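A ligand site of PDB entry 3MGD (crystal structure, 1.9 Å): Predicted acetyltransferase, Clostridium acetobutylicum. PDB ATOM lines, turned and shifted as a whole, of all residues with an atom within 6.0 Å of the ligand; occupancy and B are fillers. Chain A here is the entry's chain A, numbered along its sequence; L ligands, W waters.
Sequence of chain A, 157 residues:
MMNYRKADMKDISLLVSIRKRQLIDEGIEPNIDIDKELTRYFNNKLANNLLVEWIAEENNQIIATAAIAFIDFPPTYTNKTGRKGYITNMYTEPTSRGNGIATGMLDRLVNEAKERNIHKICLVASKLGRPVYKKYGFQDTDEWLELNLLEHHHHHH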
ATOM      1  N   GLN A  22     -17.732  30.856  -1.442  1.00  0.00           N
ATOM      2  CA  GLN A  22     -18.979  30.140  -1.649  1.00  0.00           C
ATOM      3  C   GLN A  22     -20.152  30.834  -0.971  1.00  0.00           C
ATOM      4  O   GLN A  22     -21.190  31.058  -1.583  1.00  0.00           O
ATOM      5  CB  GLN A  22     -18.827  28.722  -1.095  1.00  0.00           C
ATOM      6  CG  GLN A  22     -20.100  27.904  -1.136  1.00  0.00           C
ATOM      7  CD  GLN A  22     -20.019  26.773  -0.140  1.00  0.00           C
ATOM      8  OE1 GLN A  22     -18.925  26.239   0.101  1.00  0.00           O
ATOM      9  NE2 GLN A  22     -21.167  26.391   0.437  1.00  0.00           N
ATOM     10  N   LEU A  23     -19.979  31.191   0.292  1.00  0.00           N
ATOM     11  CA  LEU A  23     -21.058  31.801   1.049  1.00  0.00           C
ATOM     12  C   LEU A  23     -21.419  33.155   0.461  1.00  0.00           C
ATOM     13  O   LEU A  23     -22.581  33.532   0.404  1.00  0.00           O
ATOM     14  CB  LEU A  23     -20.639  31.971   2.507  1.00  0.00           C
ATOM     15  CG  LEU A  23     -20.384  30.684   3.299  1.00  0.00           C
ATOM     16  CD1 LEU A  23     -19.806  31.026   4.652  1.00  0.00           C
ATOM     17  CD2 LEU A  23     -21.676  29.843   3.452  1.00  0.00           C
ATOM     18  N   ASP A  25     -20.992  34.088  -2.667  1.00  0.00           N
ATOM     19  CA  ASP A  25     -21.712  33.708  -3.893  1.00  0.00           C
ATOM     20  C   ASP A  25     -23.187  33.369  -3.593  1.00  0.00           C
ATOM     21  O   ASP A  25     -24.076  33.659  -4.408  1.00  0.00           O
ATOM     22  CB  ASP A  25     -21.006  32.489  -4.511  1.00  0.00           C
ATOM     23  CG  ASP A  25     -20.987  32.517  -6.036  1.00  0.00           C
ATOM     24  OD1 ASP A  25     -21.918  33.100  -6.628  1.00  0.00           O
ATOM     25  OD2 ASP A  25     -20.042  31.947  -6.636  1.00  0.00           O
ATOM     26  N   GLU A  26     -23.446  32.762  -2.441  1.00  0.00           N
ATOM     27  CA  GLU A  26     -24.823  32.416  -2.047  1.00  0.00           C
ATOM     28  C   GLU A  26     -25.648  33.625  -1.597  1.00  0.00           C
ATOM     29  O   GLU A  26     -26.847  33.502  -1.368  1.00  0.00           O
ATOM     30  CB  GLU A  26     -24.820  31.368  -0.922  1.00  0.00           C
ATOM     31  CG  GLU A  26     -24.283  30.000  -1.329  1.00  0.00           C
ATOM     32  CD  GLU A  26     -24.156  29.030  -0.164  1.00  0.00           C
ATOM     33  OE1 GLU A  26     -24.984  29.117   0.776  1.00  0.00           O
ATOM     34  OE2 GLU A  26     -23.236  28.191  -0.180  1.00  0.00           O
ATOM     35  N   THR A  65     -15.040  22.226  -4.813  1.00  0.00           N
ATOM     36  CA  THR A  65     -14.914  21.514  -3.548  1.00  0.00           C
ATOM     37  C   THR A  65     -16.260  20.867  -3.226  1.00  0.00           C
ATOM     38  O   THR A  65     -17.288  21.234  -3.798  1.00  0.00           O
ATOM     39  CB  THR A  65     -14.591  22.484  -2.395  1.00  0.00           C
ATOM     40  OG1 THR A  65     -15.660  23.425  -2.243  1.00  0.00           O
ATOM     41  CG2 THR A  65     -13.282  23.230  -2.645  1.00  0.00           C
ATOM     42  N   ILE A  87     -23.756  16.945   4.148  1.00  0.00           N
ATOM     43  CA  ILE A  87     -23.027  17.451   2.993  1.00  0.00           C
ATOM     44  C   ILE A  87     -22.966  18.971   3.015  1.00  0.00           C
ATOM     45  O   ILE A  87     -23.937  19.651   3.360  1.00  0.00           O
ATOM     46  CB  ILE A  87     -23.627  16.894   1.678  1.00  0.00           C
ATOM     47  CG1 ILE A  87     -23.266  15.389   1.598  1.00  0.00           C
ATOM     48  CG2 ILE A  87     -23.174  17.721   0.470  1.00  0.00           C
ATOM     49  CD1 ILE A  87     -23.641  14.720   0.296  1.00  0.00           C
ATOM     50  N   THR A  88     -21.803  19.514   2.656  1.00  0.00           N
ATOM     51  CA  THR A  88     -21.547  20.932   2.860  1.00  0.00           C
ATOM     52  C   THR A  88     -20.360  21.375   1.999  1.00  0.00           C
ATOM     53  O   THR A  88     -19.736  20.542   1.343  1.00  0.00           O
ATOM     54  CB  THR A  88     -21.270  21.194   4.377  1.00  0.00           C
ATOM     55  OG1 THR A  88     -21.296  22.594   4.651  1.00  0.00           O
ATOM     56  CG2 THR A  88     -19.930  20.574   4.825  1.00  0.00           C
ATOM     57  N   ASN A  89     -20.053  22.674   2.037  1.00  0.00           N
ATOM     58  CA  ASN A  89     -18.878  23.204   1.378  1.00  0.00           C
ATOM     59  C   ASN A  89     -18.820  22.829  -0.090  1.00  0.00           C
ATOM     60  O   ASN A  89     -17.751  22.545  -0.618  1.00  0.00           O
ATOM     61  CB  ASN A  89     -17.596  22.740   2.079  1.00  0.00           C
ATOM     62  CG  ASN A  89     -17.469  23.287   3.479  1.00  0.00           C
ATOM     63  OD1 ASN A  89     -18.275  24.119   3.897  1.00  0.00           O
ATOM     64  ND2 ASN A  89     -16.483  22.792   4.226  1.00  0.00           N
ATOM     65  N   MET A  90     -19.960  22.807  -0.765  1.00  0.00           N
ATOM     66  CA  MET A  90     -19.943  22.548  -2.185  1.00  0.00           C
ATOM     67  C   MET A  90     -19.850  23.838  -2.984  1.00  0.00           C
ATOM     68  O   MET A  90     -20.632  24.771  -2.806  1.00  0.00           O
ATOM     69  CB  MET A  90     -21.120  21.693  -2.614  1.00  0.00           C
ATOM     70  CG  MET A  90     -21.061  20.295  -1.960  1.00  0.00           C
ATOM     71  SD  MET A  90     -22.353  19.109  -2.755  1.00  0.00           S
ATOM     72  CE  MET A  90     -21.610  19.011  -4.564  1.00  0.00           C
ATOM     73  N   TYR A  91     -18.886  23.872  -3.881  1.00  0.00           N
ATOM     74  CA  TYR A  91     -18.647  25.062  -4.693  1.00  0.00           C
ATOM     75  C   TYR A  91     -18.023  24.598  -5.995  1.00  0.00           C
ATOM     76  O   TYR A  91     -17.132  23.747  -5.990  1.00  0.00           O
ATOM     77  CB  TYR A  91     -17.732  26.049  -3.968  1.00  0.00           C
ATOM     78  CG  TYR A  91     -17.511  27.319  -4.787  1.00  0.00           C
ATOM     79  CD1 TYR A  91     -18.437  28.349  -4.757  1.00  0.00           C
ATOM     80  CD2 TYR A  91     -16.411  27.456  -5.593  1.00  0.00           C
ATOM     81  CE1 TYR A  91     -18.256  29.515  -5.528  1.00  0.00           C
ATOM     82  CE2 TYR A  91     -16.211  28.598  -6.366  1.00  0.00           C
ATOM     83  CZ  TYR A  91     -17.130  29.626  -6.331  1.00  0.00           C
ATOM     84  OH  TYR A  91     -16.911  30.758  -7.102  1.00  0.00           O
ATOM     85  N   THR A  92     -18.548  25.099  -7.105  1.00  0.00           N
ATOM     86  CA  THR A  92     -17.903  24.908  -8.395  1.00  0.00           C
ATOM     87  C   THR A  92     -17.630  26.292  -9.001  1.00  0.00           C
ATOM     88  O   THR A  92     -18.515  27.158  -8.988  1.00  0.00           O
ATOM     89  CB  THR A  92     -18.787  24.099  -9.369  1.00  0.00           C
ATOM     90  OG1 THR A  92     -19.009  22.778  -8.869  1.00  0.00           O
ATOM     91  CG2 THR A  92     -18.091  24.021 -10.759  1.00  0.00           C
ATOM     92  N   GLU A  93     -16.427  26.491  -9.528  1.00  0.00           N
ATOM     93  CA  GLU A  93     -16.052  27.722 -10.221  1.00  0.00           C
ATOM     94  C   GLU A  93     -17.128  28.035 -11.254  1.00  0.00           C
ATOM     95  O   GLU A  93     -17.541  27.154 -12.000  1.00  0.00           O
ATOM     96  CB  GLU A  93     -14.702  27.529 -10.915  1.00  0.00           C
ATOM     97  CG  GLU A  93     -14.178  28.753 -11.655  1.00  0.00           C
ATOM     98  CD  GLU A  93     -13.792  29.878 -10.698  1.00  0.00           C
ATOM     99  OE1 GLU A  93     -13.067  29.609  -9.726  1.00  0.00           O
ATOM    100  OE2 GLU A  93     -14.231  31.023 -10.937  1.00  0.00           O
ATOM    101  N   SER A  96     -17.089  26.845 -14.749  1.00  0.00           N
ATOM    102  CA  SER A  96     -17.060  25.388 -14.822  1.00  0.00           C
ATOM    103  C   SER A  96     -18.404  24.742 -14.463  1.00  0.00           C
ATOM    104  O   SER A  96     -18.528  23.515 -14.482  1.00  0.00           O
ATOM    105  CB  SER A  96     -15.973  24.833 -13.895  1.00  0.00           C
ATOM    106  OG  SER A  96     -14.666  25.039 -14.407  1.00  0.00           O
ATOM    107  N   ARG A  97     -19.397  25.550 -14.132  1.00  0.00           N
ATOM    108  CA  ARG A  97     -20.698  25.011 -13.746  1.00  0.00           C
ATOM    109  C   ARG A  97     -21.463  24.368 -14.900  1.00  0.00           C
ATOM    110  O   ARG A  97     -21.175  24.623 -16.069  1.00  0.00           O
ATOM    111  CB  ARG A  97     -21.531  26.114 -13.083  1.00  0.00           C
ATOM    112  CG  ARG A  97     -20.984  26.468 -11.713  1.00  0.00           C
ATOM    113  CD  ARG A  97     -21.658  27.681 -11.090  1.00  0.00           C
ATOM    114  NE  ARG A  97     -20.865  28.135  -9.943  1.00  0.00           N
ATOM    115  CZ  ARG A  97     -21.107  29.214  -9.220  1.00  0.00           C
ATOM    116  NH1 ARG A  97     -22.140  29.986  -9.510  1.00  0.00           N
ATOM    117  NH2 ARG A  97     -20.312  29.529  -8.209  1.00  0.00           N
ATOM    118  N   GLY A  98     -22.441  23.526 -14.565  1.00  0.00           N
ATOM    119  CA  GLY A  98     -23.260  22.850 -15.571  1.00  0.00           C
ATOM    120  C   GLY A  98     -22.576  21.738 -16.353  1.00  0.00           C
ATOM    121  O   GLY A  98     -23.063  21.316 -17.405  1.00  0.00           O
ATOM    122  N   ASN A  99     -21.438  21.260 -15.841  1.00  0.00           N
ATOM    123  CA  ASN A  99     -20.729  20.174 -16.491  1.00  0.00           C
ATOM    124  C   ASN A  99     -20.850  18.859 -15.701  1.00  0.00           C
ATOM    125  O   ASN A  99     -20.311  17.831 -16.108  1.00  0.00           O
ATOM    126  CB  ASN A  99     -19.270  20.551 -16.746  1.00  0.00           C
ATOM    127  CG  ASN A  99     -19.125  21.562 -17.874  1.00  0.00           C
ATOM    128  OD1 ASN A  99     -19.624  21.347 -18.973  1.00  0.00           O
ATOM    129  ND2 ASN A  99     -18.411  22.668 -17.608  1.00  0.00           N
ATOM    130  N   GLY A 100     -21.594  18.897 -14.608  1.00  0.00           N
ATOM    131  CA  GLY A 100     -21.784  17.703 -13.798  1.00  0.00           C
ATOM    132  C   GLY A 100     -20.747  17.532 -12.707  1.00  0.00           C
ATOM    133  O   GLY A 100     -20.636  16.450 -12.105  1.00  0.00           O
ATOM    134  N   ILE A 101     -19.980  18.579 -12.420  1.00  0.00           N
ATOM    135  CA  ILE A 101     -18.929  18.463 -11.420  1.00  0.00           C
ATOM    136  C   ILE A 101     -19.480  18.232 -10.013  1.00  0.00           C
ATOM    137  O   ILE A 101     -19.082  17.285  -9.327  1.00  0.00           O
ATOM    138  CB  ILE A 101     -17.978  19.670 -11.420  1.00  0.00           C
ATOM    139  CG1 ILE A 101     -17.230  19.741 -12.756  1.00  0.00           C
ATOM    140  CG2 ILE A 101     -16.997  19.571 -10.260  1.00  0.00           C
ATOM    141  CD1 ILE A 101     -16.320  20.948 -12.848  1.00  0.00           C
ATOM    142  N   ALA A 102     -20.385  19.092  -9.579  1.00  0.00           N
ATOM    143  CA  ALA A 102     -21.026  18.908  -8.277  1.00  0.00           C
ATOM    144  C   ALA A 102     -21.745  17.550  -8.198  1.00  0.00           C
ATOM    145  O   ALA A 102     -21.662  16.878  -7.177  1.00  0.00           O
ATOM    146  CB  ALA A 102     -21.980  20.072  -7.978  1.00  0.00           C
ATOM    147  N   THR A 103     -22.420  17.141  -9.275  1.00  0.00           N
ATOM    148  CA  THR A 103     -23.116  15.848  -9.277  1.00  0.00           C
ATOM    149  C   THR A 103     -22.149  14.663  -9.081  1.00  0.00           C
ATOM    150  O   THR A 103     -22.432  13.736  -8.315  1.00  0.00           O
ATOM    151  CB  THR A 103     -23.961  15.657 -10.574  1.00  0.00           C
ATOM    152  OG1 THR A 103     -24.988  16.656 -10.616  1.00  0.00           O
ATOM    153  CG2 THR A 103     -24.603  14.285 -10.605  1.00  0.00           C
ATOM    154  N   GLY A 104     -21.007  14.714  -9.764  1.00  0.00           N
ATOM    155  CA  GLY A 104     -19.984  13.697  -9.588  1.00  0.00           C
ATOM    156  C   GLY A 104     -19.361  13.757  -8.201  1.00  0.00           C
ATOM    157  O   GLY A 104     -18.972  12.729  -7.643  1.00  0.00           O
ATOM    158  N   LEU A 123     -28.509  17.698   4.137  1.00  0.00           N
ATOM    159  CA  LEU A 123     -27.821  18.931   3.786  1.00  0.00           C
ATOM    160  C   LEU A 123     -28.805  20.082   3.854  1.00  0.00           C
ATOM    161  O   LEU A 123     -30.015  19.871   3.933  1.00  0.00           O
ATOM    162  CB  LEU A 123     -27.217  18.839   2.379  1.00  0.00           C
ATOM    163  CG  LEU A 123     -28.148  18.501   1.201  1.00  0.00           C
ATOM    164  CD1 LEU A 123     -29.076  19.655   0.827  1.00  0.00           C
ATOM    165  CD2 LEU A 123     -27.332  18.077   0.004  1.00  0.00           C
ATOM    166  N   VAL A 124     -28.273  21.299   3.823  1.00  0.00           N
ATOM    167  CA  VAL A 124     -29.090  22.499   3.668  1.00  0.00           C
ATOM    168  C   VAL A 124     -28.874  23.058   2.266  1.00  0.00           C
ATOM    169  O   VAL A 124     -27.765  23.427   1.882  1.00  0.00           O
ATOM    170  CB  VAL A 124     -28.725  23.572   4.711  1.00  0.00           C
ATOM    171  CG1 VAL A 124     -29.514  24.856   4.438  1.00  0.00           C
ATOM    172  CG2 VAL A 124     -28.985  23.051   6.145  1.00  0.00           C
ATOM    173  N   ALA A 125     -29.945  23.126   1.488  1.00  0.00           N
ATOM    174  CA  ALA A 125     -29.836  23.464   0.081  1.00  0.00           C
ATOM    175  C   ALA A 125     -29.803  24.967  -0.137  1.00  0.00           C
ATOM    176  O   ALA A 125     -30.651  25.703   0.375  1.00  0.00           O
ATOM    177  CB  ALA A 125     -30.994  22.844  -0.688  1.00  0.00           C
ATOM    178  N   SER A 126     -28.816  25.422  -0.888  1.00  0.00           N
ATOM    179  CA  SER A 126     -28.753  26.807  -1.333  1.00  0.00           C
ATOM    180  C   SER A 126     -29.627  26.957  -2.580  1.00  0.00           C
ATOM    181  O   SER A 126     -30.148  25.953  -3.081  1.00  0.00           O
ATOM    182  CB  SER A 126     -27.327  27.168  -1.680  1.00  0.00           C
ATOM    183  OG  SER A 126     -26.909  26.389  -2.782  1.00  0.00           O
ATOM    184  N   LYS A 127     -29.766  28.180  -3.082  1.00  0.00           N
ATOM    185  CA  LYS A 127     -30.591  28.433  -4.274  1.00  0.00           C
ATOM    186  C   LYS A 127     -30.095  27.659  -5.497  1.00  0.00           C
ATOM    187  O   LYS A 127     -30.894  27.103  -6.257  1.00  0.00           O
ATOM    188  CB  LYS A 127     -30.637  29.925  -4.606  1.00  0.00           C
ATOM    189  CG  LYS A 127     -31.645  30.711  -3.791  1.00  0.00           C
ATOM    190  CD  LYS A 127     -31.730  32.159  -4.262  1.00  0.00           C
ATOM    191  CE  LYS A 127     -32.088  32.253  -5.735  1.00  0.00           C
ATOM    192  NZ  LYS A 127     -32.294  33.669  -6.186  1.00  0.00           N
ATOM    193  N   LEU A 128     -28.781  27.668  -5.694  1.00  0.00           N
ATOM    194  CA  LEU A 128     -28.199  26.994  -6.845  1.00  0.00           C
ATOM    195  C   LEU A 128     -28.041  25.504  -6.593  1.00  0.00           C
ATOM    196  O   LEU A 128     -28.032  24.699  -7.523  1.00  0.00           O
ATOM    197  CB  LEU A 128     -26.839  27.616  -7.183  1.00  0.00           C
ATOM    198  CG  LEU A 128     -26.944  29.002  -7.810  1.00  0.00           C
ATOM    199  CD1 LEU A 128     -25.579  29.680  -7.931  1.00  0.00           C
ATOM    200  CD2 LEU A 128     -27.609  28.886  -9.179  1.00  0.00           C
ATOM    201  N   GLY A 129     -27.908  25.141  -5.332  1.00  0.00           N
ATOM    202  CA  GLY A 129     -27.687  23.761  -4.985  1.00  0.00           C
ATOM    203  C   GLY A 129     -28.944  22.941  -5.132  1.00  0.00           C
ATOM    204  O   GLY A 129     -28.880  21.775  -5.499  1.00  0.00           O
ATOM    205  N   PRO A 131     -31.821  22.445  -7.083  1.00  0.00           N
ATOM    206  CA  PRO A 131     -32.148  21.617  -8.252  1.00  0.00           C
ATOM    207  C   PRO A 131     -31.130  20.495  -8.475  1.00  0.00           C
ATOM    208  O   PRO A 131     -31.493  19.433  -8.985  1.00  0.00           O
ATOM    209  CB  PRO A 131     -32.085  22.599  -9.420  1.00  0.00           C
ATOM    210  CG  PRO A 131     -31.958  23.964  -8.822  1.00  0.00           C
ATOM    211  CD  PRO A 131     -31.378  23.792  -7.470  1.00  0.00           C
ATOM    212  N   VAL A 132     -29.869  20.731  -8.135  1.00  0.00           N
ATOM    213  CA  VAL A 132     -28.852  19.674  -8.224  1.00  0.00           C
ATOM    214  C   VAL A 132     -29.168  18.524  -7.269  1.00  0.00           C
ATOM    215  O   VAL A 132     -29.159  17.353  -7.668  1.00  0.00           O
ATOM    216  CB  VAL A 132     -27.440  20.218  -7.903  1.00  0.00           C
ATOM    217  CG1 VAL A 132     -26.397  19.133  -8.088  1.00  0.00           C
ATOM    218  CG2 VAL A 132     -27.135  21.409  -8.800  1.00  0.00           C
ATOM    219  N   TYR A 133     -29.460  18.864  -6.014  1.00  0.00           N
ATOM    220  CA  TYR A 133     -29.782  17.857  -5.013  1.00  0.00           C
ATOM    221  C   TYR A 133     -31.125  17.192  -5.292  1.00  0.00           C
ATOM    222  O   TYR A 133     -31.267  15.988  -5.095  1.00  0.00           O
ATOM    223  CB  TYR A 133     -29.736  18.463  -3.609  1.00  0.00           C
ATOM    224  CG  TYR A 133     -28.462  19.248  -3.371  1.00  0.00           C
ATOM    225  CD1 TYR A 133     -27.241  18.741  -3.809  1.00  0.00           C
ATOM    226  CD2 TYR A 133     -28.476  20.484  -2.752  1.00  0.00           C
ATOM    227  CE1 TYR A 133     -26.069  19.457  -3.620  1.00  0.00           C
ATOM    228  CE2 TYR A 133     -27.313  21.196  -2.552  1.00  0.00           C
ATOM    229  CZ  TYR A 133     -26.106  20.671  -2.996  1.00  0.00           C
ATOM    230  OH  TYR A 133     -24.923  21.378  -2.811  1.00  0.00           O
ATOM    231  N   LYS A 135     -32.476  16.784  -8.267  1.00  0.00           N
ATOM    232  CA  LYS A 135     -32.191  15.891  -9.390  1.00  0.00           C
ATOM    233  C   LYS A 135     -31.530  14.600  -8.917  1.00  0.00           C
ATOM    234  O   LYS A 135     -31.821  13.513  -9.419  1.00  0.00           O
ATOM    235  CB  LYS A 135     -31.347  16.592 -10.469  1.00  0.00           C
ATOM    236  CG  LYS A 135     -31.047  15.735 -11.696  1.00  0.00           C
ATOM    237  CD  LYS A 135     -30.089  16.449 -12.636  1.00  0.00           C
ATOM    238  CE  LYS A 135     -29.958  15.737 -13.988  1.00  0.00           C
ATOM    239  NZ  LYS A 135     -28.753  16.196 -14.752  1.00  0.00           N
HETATM  240  N1  LIG L   1     -26.518  16.262 -18.785  1.00  0.00           N
HETATM  241  C1  LIG L   1     -27.422  17.326 -18.792  1.00  0.00           C
HETATM  242  N2  LIG L   1     -27.336  18.349 -17.821  1.00  0.00           N
HETATM  243  C2  LIG L   1     -26.292  18.280 -16.803  1.00  0.00           C
HETATM  244  C3  LIG L   1     -25.356  17.197 -16.797  1.00  0.00           C
HETATM  245  C4  LIG L   1     -25.453  16.190 -17.744  1.00  0.00           C
HETATM  246  N3  LIG L   1     -24.505  15.093 -17.725  1.00  0.00           N
HETATM  247  N4  LIG L   1     -24.450  17.385 -15.698  1.00  0.00           N
HETATM  248  C5  LIG L   1     -24.809  18.563 -15.048  1.00  0.00           C
HETATM  249  N5  LIG L   1     -25.972  19.122 -15.734  1.00  0.00           N
HETATM  250  C6  LIG L   1     -26.556  20.411 -15.410  1.00  0.00           C
HETATM  251  C7  LIG L   1     -27.677  20.042 -14.418  1.00  0.00           C
HETATM  252  O1  LIG L   1     -28.702  19.166 -14.770  1.00  0.00           O
HETATM  253  C8  LIG L   1     -28.007  21.382 -13.808  1.00  0.00           C
HETATM  254  O2  LIG L   1     -28.930  22.220 -14.456  1.00  0.00           O
HETATM  255  P1  LIG L   1     -30.490  22.228 -14.109  1.00  0.00           P
HETATM  256  O3  LIG L   1     -31.253  22.820 -15.338  1.00  0.00           O
HETATM  257  O4  LIG L   1     -30.746  23.105 -12.863  1.00  0.00           O
HETATM  258  O5  LIG L   1     -30.984  20.819 -13.829  1.00  0.00           O
HETATM  259  C9  LIG L   1     -26.557  21.953 -13.612  1.00  0.00           C
HETATM  260  O6  LIG L   1     -25.845  21.522 -14.823  1.00  0.00           O
HETATM  261  C10 LIG L   1     -25.789  21.885 -12.310  1.00  0.00           C
HETATM  262  O7  LIG L   1     -25.330  20.579 -12.049  1.00  0.00           O
HETATM  263  P2  LIG L   1     -23.798  20.301 -11.787  1.00  0.00           P
HETATM  264  O8  LIG L   1     -22.929  20.614 -13.012  1.00  0.00           O
HETATM  265  O9  LIG L   1     -23.673  18.851 -11.324  1.00  0.00           O
HETATM  266  O10 LIG L   1     -23.418  21.246 -10.582  1.00  0.00           O
HETATM  267  P3  LIG L   1     -22.285  22.373 -10.643  1.00  0.00           P
HETATM  268  O11 LIG L   1     -22.626  23.532 -11.639  1.00  0.00           O
HETATM  269  O12 LIG L   1     -20.930  21.758 -10.882  1.00  0.00           O
HETATM  270  O13 LIG L   1     -22.186  22.946  -9.184  1.00  0.00           O
HETATM  271  C11 LIG L   1     -23.106  24.242  -7.338  1.00  0.00           C
HETATM  272  C12 LIG L   1     -23.359  23.271  -8.486  1.00  0.00           C
HETATM  273  C13 LIG L   1     -24.344  24.374  -6.483  1.00  0.00           C
HETATM  274  C14 LIG L   1     -21.944  23.723  -6.552  1.00  0.00           C
HETATM  275  C15 LIG L   1     -22.770  25.647  -7.956  1.00  0.00           C
HETATM  276  O14 LIG L   1     -23.835  26.171  -8.680  1.00  0.00           O
HETATM  277  C16 LIG L   1     -22.154  26.631  -6.991  1.00  0.00           C
HETATM  278  O15 LIG L   1     -20.971  26.582  -6.655  1.00  0.00           O
HETATM  279  N6  LIG L   1     -23.028  27.668  -6.492  1.00  0.00           N
HETATM  280  C17 LIG L   1     -22.558  28.622  -5.506  1.00  0.00           C
HETATM  281  C18 LIG L   1     -22.248  27.977  -4.206  1.00  0.00           C
HETATM  282  C19 LIG L   1     -23.366  27.078  -3.756  1.00  0.00           C
HETATM  283  O16 LIG L   1     -24.544  27.461  -3.824  1.00  0.00           O
HETATM  284  N7  LIG L   1     -23.027  25.769  -3.305  1.00  0.00           N
HETATM  285  C20 LIG L   1     -23.983  24.925  -2.633  1.00  0.00           C
HETATM  286  C21 LIG L   1     -24.242  25.227  -1.177  1.00  0.00           C
HETATM  287  S1  LIG L   1     -25.304  24.058  -0.371  1.00  0.00           S
HETATM  288  C22 LIG L   1     -24.458  22.702   0.146  1.00  0.00           C
HETATM  289  O17 LIG L   1     -23.253  22.633  -0.036  1.00  0.00           O
HETATM  290  C23 LIG L   1     -25.198  21.539   0.694  1.00  0.00           C
HETATM  291  O   HOH W   1     -19.821  21.444 -13.392  1.00  0.00           O
HETATM  292  O   HOH W   2     -24.786  24.147   3.121  1.00  0.00           O
HETATM  293  O   HOH W   3     -25.621  21.815   4.027  1.00  0.00           O
HETATM  294  O   HOH W   4     -26.574  29.256  -4.270  1.00  0.00           O
HETATM  295  O   HOH W   5     -24.369  15.153 -14.186  1.00  0.00           O
HETATM  296  O   HOH W   6     -24.633  25.318 -11.107  1.00  0.00           O
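The backbone carbonyl oxygen (O) of Val 124 lies close to a sulfur (S1) of the ligand (3.4 Å).
Residues that only touch the ligand: Glu 26, Tyr 91, Ile 87, Leu 128, Ile 101, Gln 22, Gly 129, Pro 131, Thr 88, Leu 123, Val 132 and Asn 89.
Hydrophobic or aromatic side chains within 4 Å of the ligand: Met 90, Tyr 91, Ile 101, Ala 102, Leu 123, Leu 128, Pro 131, Val 132 and Tyr 133.
24 residues have an atom within 4 Å of the ligand: Gln 22, Glu 26, Ile 87, Thr 88, Asn 89, Met 90, Tyr 91, Thr 92, Arg 97, Gly 98, Asn 99, Gly 100, Ile 101, Ala 102, Thr 103, Leu 123, Val 124, Ser 126, Leu 128, Gly 129, Pro 131, Val 132, Tyr 133 and Lys 135.
O17 of the ligand lies within hydrogen-bond range of N of Met 90.
A nitrogen (N7) of the ligand lies within hydrogen-bond range of the backbone carbonyl oxygen (O) of Met 90, 2.6 Å away.
O9 of the ligand sits at hydrogen-bond distance from N of Thr 103 (2.9 Å).
The side-chain hydroxyl of Thr 103 is in hydrogen-bond range of an oxygen (O9) of the ligand.
The backbone NH (N) of Gly 100 lies within hydrogen-bond range of an oxygen (O8) of the ligand, 2.7 Å away.
The side-chain hydroxyl of Ser 126 is in hydrogen-bond range of an oxygen (O16) of the ligand (2.8 Å).
O15 of the ligand sits at hydrogen-bond distance from N of Thr 92 (2.9 Å).
The side-chain hydroxyl (OG1) of Thr 92 sits at hydrogen-bond distance from an oxygen (O12) of the ligand, 3.0 Å away.
The backbone NH (N) of Gly 98 is in hydrogen-bond range of an oxygen (O11) of the ligand, 2.9 Å away.
An oxygen (O1) of the ligand sits at hydrogen-bond distance from the side-chain amino group of Lys 135, at 3.0 Å.
The backbone NH (N) of Ala 102 is in hydrogen-bond range of an oxygen (O12) of the ligand.
The guanidinium group (NH2) of Arg 97 lies within hydrogen-bond range of an oxygen (O15) of the ligand.
N of Asn 99 is in hydrogen-bond range of O8 of the ligand, 3.3 Å away.
OH of Tyr 133 sits close to O17 of the ligand.
Water W4 lies within hydrogen-bond range of an oxygen (O16) of the ligand (2.7 Å), the backbone NH (N) of Leu 128 (3.1 Å) and the side-chain hydroxyl (OG) of Ser 126 (3.2 Å).
Water W2 lies within hydrogen-bond range of the backbone carbonyl oxygen of Val 124 and a sulfur (S1) of the ligand.
Water W3 lies within hydrogen-bond range of N of Val 124 (2.7 Å) and O of Ile 87 (2.8 Å).
The side-chain sulfur of Met 90 lies within hydrogen-bond range of the side-chain hydroxyl of Tyr 133, at 3.4 Å.
The backbone NH of Gly 129 is in hydrogen-bond range of the side-chain hydroxyl of Ser 126, at 3.0 Å.
The guanidinium group (NH2) of Arg 97 is in salt-bridge range of the side-chain carboxylate (OD2) of Asp 25 (2.9 Å).
The side-chain amide nitrogen (ND2) of Asn 99 sits at hydrogen-bond distance from the backbone carbonyl oxygen (O) of Ser 96, at 3.2 Å.
The side-chain amide nitrogen (NE2) of Gln 22 sits at hydrogen-bond distance from the side-chain carboxylate (OE2) of Glu 26 (2.8 Å).
The side-chain hydroxyl of Tyr 91 lies close to the side-chain carboxylate of Asp 25, 3.4 Å away.
The side-chain hydroxyl (OG1) of Thr 88 sits at hydrogen-bond distance from the side-chain amide oxygen (OD1) of Asn 89.
OG1 of Thr 65 sits at hydrogen-bond distance from O of Asn 89 (2.8 Å).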
